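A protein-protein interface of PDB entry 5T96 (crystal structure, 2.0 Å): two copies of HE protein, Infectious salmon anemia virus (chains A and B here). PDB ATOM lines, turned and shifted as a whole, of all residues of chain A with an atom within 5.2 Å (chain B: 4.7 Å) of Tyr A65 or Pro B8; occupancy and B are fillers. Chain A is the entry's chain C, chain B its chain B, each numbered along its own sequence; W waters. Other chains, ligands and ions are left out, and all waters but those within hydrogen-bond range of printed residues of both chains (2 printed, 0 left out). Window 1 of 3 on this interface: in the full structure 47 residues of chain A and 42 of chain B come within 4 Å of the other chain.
O of Gly B36 sits at hydrogen-bond distance from NZ of Lys A64 (3.1 Å).
The backbone carbonyl oxygen (O) of Tyr B7 lies close to the backbone NH (N) of Gly B36, 3.5 Å away. NE of Arg A5 lies within salt-bridge range of OD1 of Asp A9. The backbone carbonyl oxygen (O) of Asp A9 is in hydrogen-bond range of the backbone NH (N) of Tyr A65 (3.2 Å). N of Thr A11 sits at hydrogen-bond distance from O of Tyr A65, 2.9 Å away. The side-chain hydroxyl (OG1) of Thr A63 lies within hydrogen-bond range of the backbone carbonyl oxygen (O) of Tyr A65 (2.8 Å). The side-chain hydroxyl (OH) of Tyr A65 lies within hydrogen-bond range of the side-chain carboxylate (OD1) of Asp A272, at 2.6 Å.
OD2 of Asp A9 touches CG of Pro B8, at 3.7 Å. Lys B35 touches Lys A64 (O to CE, 3.4 Å). Pro B8 touches Tyr A65. Lys B35 touches Asp A272 (CG to OD2, 3.9 Å).
Of the printed residues of chain B, Asp A9 touches Pro B8. Thr A63 touches none of the printed residues of chain B. Printed residues of chain B within 4 Å of Lys A64: Lys B35 (3.4 Å) and Gly B36 (3.1 Å). Of chain B, only Pro B8 comes within 4 Å of Tyr A65. Pro B8 touches just these residues of chain A: Asp A9 (3.7 Å) and Tyr A65 (3.9 Å). Printed residues of chain A within 4 Å of Lys B35: Lys A64 and Asp A272. The nearest residue of chain B that does not touch Tyr A65 is Lys B35 (4.1 Å).
Hydrophobic or aromatic side chains of chain A within 4 Å of the printed part of chain B: Tyr A65. Of the 7 printed residues of chain B, 3 touch a printed residue of chain A. Printed residues of chain B that touch a printed residue of chain A: Pro B8, Lys B35 and Gly B36. Among the printed residues, no Asp or Glu carboxylate lies within 4 Å of a Lys or Arg side-chain nitrogen of the other chain.
Positions printed for both chains: 9, 10 and 63.
Water W1 bridges O of Pro B8 and N of Lys A64. Water W2 bridges NZ of Lys A64 (3.0 Å) and O of Gly B36 (3.0 Å).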
ATOM      1  N   ARG A   5       6.287 -20.686  29.595  1.00  0.00           N
ATOM      2  CA  ARG A   5       7.481 -19.913  29.898  1.00  0.00           C
ATOM      3  C   ARG A   5       7.622 -18.741  28.932  1.00  0.00           C
ATOM      4  O   ARG A   5       7.872 -18.928  27.741  1.00  0.00           O
ATOM      5  CB  ARG A   5       8.726 -20.784  29.841  1.00  0.00           C
ATOM      6  CG  ARG A   5       9.944 -20.138  30.500  1.00  0.00           C
ATOM      7  CD  ARG A   5      11.155 -21.035  30.391  1.00  0.00           C
ATOM      8  NE  ARG A   5      12.293 -20.455  31.073  1.00  0.00           N
ATOM      9  CZ  ARG A   5      12.605 -20.681  32.338  1.00  0.00           C
ATOM     10  NH1 ARG A   5      11.849 -21.498  33.073  1.00  0.00           N
ATOM     11  NH2 ARG A   5      13.672 -20.085  32.867  1.00  0.00           N
ATOM     12  N   ASP A   9      15.090 -16.970  27.748  1.00  0.00           N
ATOM     13  CA  ASP A   9      15.781 -18.234  27.508  1.00  0.00           C
ATOM     14  C   ASP A   9      14.905 -19.248  26.805  1.00  0.00           C
ATOM     15  O   ASP A   9      15.176 -20.458  26.871  1.00  0.00           O
ATOM     16  CB  ASP A   9      16.286 -18.822  28.819  1.00  0.00           C
ATOM     17  CG  ASP A   9      15.172 -19.010  29.835  1.00  0.00           C
ATOM     18  OD1 ASP A   9      13.965 -18.964  29.464  1.00  0.00           O
ATOM     19  OD2 ASP A   9      15.520 -19.199  31.012  1.00  0.00           O
ATOM     20  N   THR A  10      13.863 -18.775  26.144  1.00  0.00           N
ATOM     21  CA  THR A  10      12.858 -19.586  25.488  1.00  0.00           C
ATOM     22  C   THR A  10      12.733 -19.145  24.037  1.00  0.00           C
ATOM     23  O   THR A  10      12.739 -17.941  23.740  1.00  0.00           O
ATOM     24  CB  THR A  10      11.521 -19.432  26.245  1.00  0.00           C
ATOM     25  OG1 THR A  10      11.750 -19.729  27.621  1.00  0.00           O
ATOM     26  CG2 THR A  10      10.455 -20.351  25.724  1.00  0.00           C
ATOM     27  N   THR A  11      12.648 -20.119  23.132  1.00  0.00           N
ATOM     28  CA  THR A  11      12.402 -19.861  21.714  1.00  0.00           C
ATOM     29  C   THR A  11      11.028 -20.368  21.332  1.00  0.00           C
ATOM     30  O   THR A  11      10.695 -21.529  21.592  1.00  0.00           O
ATOM     31  CB  THR A  11      13.467 -20.517  20.827  1.00  0.00           C
ATOM     32  OG1 THR A  11      14.760 -20.017  21.189  1.00  0.00           O
ATOM     33  CG2 THR A  11      13.209 -20.232  19.327  1.00  0.00           C
ATOM     34  N   THR A  63      18.419 -21.841  22.623  1.00  0.00           N
ATOM     35  CA  THR A  63      18.057 -21.676  24.021  1.00  0.00           C
ATOM     36  C   THR A  63      17.729 -23.008  24.675  1.00  0.00           C
ATOM     37  O   THR A  63      17.367 -23.992  24.019  1.00  0.00           O
ATOM     38  CB  THR A  63      16.837 -20.753  24.167  1.00  0.00           C
ATOM     39  OG1 THR A  63      15.748 -21.261  23.375  1.00  0.00           O
ATOM     40  CG2 THR A  63      17.179 -19.329  23.754  1.00  0.00           C
ATOM     41  N   LYS A  64      17.825 -23.008  26.005  1.00  0.00           N
ATOM     42  CA  LYS A  64      17.437 -24.173  26.801  1.00  0.00           C
ATOM     43  C   LYS A  64      15.982 -24.573  26.574  1.00  0.00           C
ATOM     44  O   LYS A  64      15.665 -25.770  26.522  1.00  0.00           O
ATOM     45  CB  LYS A  64      17.667 -23.877  28.282  1.00  0.00           C
ATOM     46  CG  LYS A  64      17.112 -24.930  29.258  1.00  0.00           C
ATOM     47  CD  LYS A  64      17.869 -26.243  29.150  1.00  0.00           C
ATOM     48  CE  LYS A  64      17.400 -27.253  30.189  1.00  0.00           C
ATOM     49  NZ  LYS A  64      18.287 -28.427  30.294  1.00  0.00           N
ATOM     50  N   TYR A  65      15.072 -23.598  26.482  1.00  0.00           N
ATOM     51  CA  TYR A  65      13.655 -23.896  26.446  1.00  0.00           C
ATOM     52  C   TYR A  65      13.062 -23.512  25.094  1.00  0.00           C
ATOM     53  O   TYR A  65      13.552 -22.609  24.402  1.00  0.00           O
ATOM     54  CB  TYR A  65      12.876 -23.175  27.571  1.00  0.00           C
ATOM     55  CG  TYR A  65      13.465 -23.455  28.909  1.00  0.00           C
ATOM     56  CD1 TYR A  65      13.209 -24.656  29.560  1.00  0.00           C
ATOM     57  CD2 TYR A  65      14.316 -22.538  29.529  1.00  0.00           C
ATOM     58  CE1 TYR A  65      13.776 -24.935  30.797  1.00  0.00           C
ATOM     59  CE2 TYR A  65      14.882 -22.814  30.767  1.00  0.00           C
ATOM     60  CZ  TYR A  65      14.624 -24.020  31.383  1.00  0.00           C
ATOM     61  OH  TYR A  65      15.204 -24.300  32.613  1.00  0.00           O
ATOM     62  N   ARG A  66      12.008 -24.218  24.727  1.00  0.00           N
ATOM     63  CA  ARG A  66      11.303 -23.943  23.484  1.00  0.00           C
ATOM     64  C   ARG A  66       9.817 -24.104  23.714  1.00  0.00           C
ATOM     65  O   ARG A  66       9.388 -24.841  24.606  1.00  0.00           O
ATOM     66  CB  ARG A  66      11.735 -24.876  22.306  1.00  0.00           C
ATOM     67  CG  ARG A  66      13.186 -24.753  21.904  1.00  0.00           C
ATOM     68  CD  ARG A  66      14.041 -25.749  22.717  1.00  0.00           C
ATOM     69  NE  ARG A  66      15.460 -25.520  22.563  1.00  0.00           N
ATOM     70  CZ  ARG A  66      16.239 -26.132  21.683  1.00  0.00           C
ATOM     71  NH1 ARG A  66      15.747 -27.030  20.836  1.00  0.00           N
ATOM     72  NH2 ARG A  66      17.527 -25.860  21.665  1.00  0.00           N
ATOM     73  N   ILE A  67       9.025 -23.371  22.921  1.00  0.00           N
ATOM     74  CA  ILE A  67       7.600 -23.620  22.791  1.00  0.00           C
ATOM     75  C   ILE A  67       7.301 -23.766  21.300  1.00  0.00           C
ATOM     76  O   ILE A  67       7.626 -22.873  20.508  1.00  0.00           O
ATOM     77  CB  ILE A  67       6.751 -22.497  23.407  1.00  0.00           C
ATOM     78  CG1 ILE A  67       7.062 -22.315  24.889  1.00  0.00           C
ATOM     79  CG2 ILE A  67       5.276 -22.815  23.221  1.00  0.00           C
ATOM     80  CD1 ILE A  67       6.514 -21.038  25.428  1.00  0.00           C
ATOM     81  N   LYS A 204      14.425 -28.562  26.674  1.00  0.00           N
ATOM     82  CA  LYS A 204      13.046 -28.828  27.097  1.00  0.00           C
ATOM     83  C   LYS A 204      12.048 -27.973  26.324  1.00  0.00           C
ATOM     84  O   LYS A 204      12.340 -26.821  25.978  1.00  0.00           O
ATOM     85  CB  LYS A 204      12.854 -28.559  28.614  1.00  0.00           C
ATOM     86  CG  LYS A 204      13.629 -29.495  29.541  1.00  0.00           C
ATOM     87  CD  LYS A 204      13.334 -29.112  31.004  1.00  0.00           C
ATOM     88  CE  LYS A 204      14.010 -30.000  32.015  1.00  0.00           C
ATOM     89  NZ  LYS A 204      13.599 -31.367  31.859  1.00  0.00           N
ATOM     90  N   ILE A 271      12.366 -22.163  38.030  1.00  0.00           N
ATOM     91  CA  ILE A 271      11.815 -23.438  37.587  1.00  0.00           C
ATOM     92  C   ILE A 271      12.491 -23.877  36.295  1.00  0.00           C
ATOM     93  O   ILE A 271      12.584 -23.104  35.330  1.00  0.00           O
ATOM     94  CB  ILE A 271      10.280 -23.399  37.421  1.00  0.00           C
ATOM     95  CG1 ILE A 271       9.782 -24.797  36.982  1.00  0.00           C
ATOM     96  CG2 ILE A 271       9.830 -22.303  36.445  1.00  0.00           C
ATOM     97  CD1 ILE A 271       8.274 -24.970  36.905  1.00  0.00           C
ATOM     98  N   ASP A 272      12.939 -25.132  36.277  1.00  0.00           N
ATOM     99  CA  ASP A 272      13.571 -25.733  35.096  1.00  0.00           C
ATOM    100  C   ASP A 272      12.488 -26.439  34.276  1.00  0.00           C
ATOM    101  O   ASP A 272      12.347 -27.665  34.254  1.00  0.00           O
ATOM    102  CB  ASP A 272      14.683 -26.682  35.515  1.00  0.00           C
ATOM    103  CG  ASP A 272      15.359 -27.393  34.312  1.00  0.00           C
ATOM    104  OD1 ASP A 272      15.360 -26.859  33.185  1.00  0.00           O
ATOM    105  OD2 ASP A 272      15.952 -28.470  34.515  1.00  0.00           O
ATOM    106  N   ALA A 273      11.690 -25.625  33.609  1.00  0.00           N
ATOM    107  CA  ALA A 273      10.604 -26.162  32.811  1.00  0.00           C
ATOM    108  C   ALA A 273      10.119 -25.091  31.867  1.00  0.00           C
ATOM    109  O   ALA A 273      10.237 -23.896  32.149  1.00  0.00           O
ATOM    110  CB  ALA A 273       9.448 -26.639  33.688  1.00  0.00           C
ATOM    111  N   ALA A 274       9.542 -25.536  30.761  1.00  0.00           N
ATOM    112  CA  ALA A 274       8.962 -24.638  29.780  1.00  0.00           C
ATOM    113  C   ALA A 274       7.524 -24.269  30.112  1.00  0.00           C
ATOM    114  O   ALA A 274       6.932 -23.439  29.400  1.00  0.00           O
ATOM    115  CB  ALA A 274       9.037 -25.291  28.395  1.00  0.00           C
ATOM    116  N   TYR B   7      22.364 -23.235  35.448  1.00  0.00           N
ATOM    117  CA  TYR B   7      21.485 -22.139  35.048  1.00  0.00           C
ATOM    118  C   TYR B   7      21.370 -22.111  33.524  1.00  0.00           C
ATOM    119  O   TYR B   7      22.288 -22.556  32.835  1.00  0.00           O
ATOM    120  CB  TYR B   7      22.049 -20.813  35.564  1.00  0.00           C
ATOM    121  CG  TYR B   7      21.054 -19.761  35.964  1.00  0.00           C
ATOM    122  CD1 TYR B   7      20.113 -19.993  36.951  1.00  0.00           C
ATOM    123  CD2 TYR B   7      21.115 -18.499  35.394  1.00  0.00           C
ATOM    124  CE1 TYR B   7      19.236 -19.004  37.331  1.00  0.00           C
ATOM    125  CE2 TYR B   7      20.257 -17.515  35.759  1.00  0.00           C
ATOM    126  CZ  TYR B   7      19.311 -17.756  36.733  1.00  0.00           C
ATOM    127  OH  TYR B   7      18.441 -16.740  37.097  1.00  0.00           O
ATOM    128  N   PRO B   8      20.262 -21.600  32.973  1.00  0.00           N
ATOM    129  CA  PRO B   8      20.050 -21.702  31.506  1.00  0.00           C
ATOM    130  C   PRO B   8      21.034 -20.903  30.655  1.00  0.00           C
ATOM    131  O   PRO B   8      21.057 -21.091  29.426  1.00  0.00           O
ATOM    132  CB  PRO B   8      18.619 -21.189  31.317  1.00  0.00           C
ATOM    133  CG  PRO B   8      17.950 -21.398  32.691  1.00  0.00           C
ATOM    134  CD  PRO B   8      19.062 -21.130  33.681  1.00  0.00           C
ATOM    135  N   ASP B   9      21.847 -20.028  31.245  1.00  0.00           N
ATOM    136  CA  ASP B   9      22.824 -19.260  30.479  1.00  0.00           C
ATOM    137  C   ASP B   9      24.198 -19.915  30.482  1.00  0.00           C
ATOM    138  O   ASP B   9      25.193 -19.254  30.180  1.00  0.00           O
ATOM    139  CB  ASP B   9      22.922 -17.827  31.011  1.00  0.00           C
ATOM    140  CG  ASP B   9      23.241 -17.767  32.511  1.00  0.00           C
ATOM    141  OD1 ASP B   9      23.647 -18.784  33.097  1.00  0.00           O
ATOM    142  OD2 ASP B   9      23.101 -16.681  33.102  1.00  0.00           O
ATOM    143  N   THR B  10      24.264 -21.204  30.788  1.00  0.00           N
ATOM    144  CA  THR B  10      25.515 -21.938  30.905  1.00  0.00           C
ATOM    145  C   THR B  10      25.457 -23.168  29.998  1.00  0.00           C
ATOM    146  O   THR B  10      24.424 -23.837  29.934  1.00  0.00           O
ATOM    147  CB  THR B  10      25.751 -22.357  32.372  1.00  0.00           C
ATOM    148  OG1 THR B  10      25.625 -21.207  33.223  1.00  0.00           O
ATOM    149  CG2 THR B  10      27.130 -22.925  32.535  1.00  0.00           C
ATOM    150  N   LYS B  35      20.574 -27.558  34.321  1.00  0.00           N
ATOM    151  CA  LYS B  35      19.566 -26.608  33.865  1.00  0.00           C
ATOM    152  C   LYS B  35      20.013 -25.798  32.665  1.00  0.00           C
ATOM    153  O   LYS B  35      19.190 -25.063  32.102  1.00  0.00           O
ATOM    154  CB  LYS B  35      19.174 -25.629  34.975  1.00  0.00           C
ATOM    155  CG  LYS B  35      18.646 -26.312  36.226  1.00  0.00           C
ATOM    156  CD  LYS B  35      18.103 -25.293  37.194  1.00  0.00           C
ATOM    157  CE  LYS B  35      17.778 -25.893  38.556  1.00  0.00           C
ATOM    158  NZ  LYS B  35      17.322 -24.823  39.490  1.00  0.00           N
ATOM    159  N   GLY B  36      21.293 -25.853  32.304  1.00  0.00           N
ATOM    160  CA  GLY B  36      21.772 -25.201  31.107  1.00  0.00           C
ATOM    161  C   GLY B  36      21.746 -26.120  29.895  1.00  0.00           C
ATOM    162  O   GLY B  36      21.132 -27.187  29.887  1.00  0.00           O
ATOM    163  N   THR B  63      26.404 -19.398  24.794  1.00  0.00           N
ATOM    164  CA  THR B  63      26.073 -18.756  26.062  1.00  0.00           C
ATOM    165  C   THR B  63      27.284 -18.037  26.677  1.00  0.00           C
ATOM    166  O   THR B  63      28.448 -18.324  26.382  1.00  0.00           O
ATOM    167  CB  THR B  63      25.560 -19.792  27.066  1.00  0.00           C
ATOM    168  OG1 THR B  63      26.539 -20.817  27.263  1.00  0.00           O
ATOM    169  CG2 THR B  63      24.287 -20.406  26.560  1.00  0.00           C
HETATM  170  O   HOH W   1      19.355 -20.888  27.272  1.00  0.00           O
HETATM  171  O   HOH W   2      20.728 -30.196  30.000  1.00  0.00           O
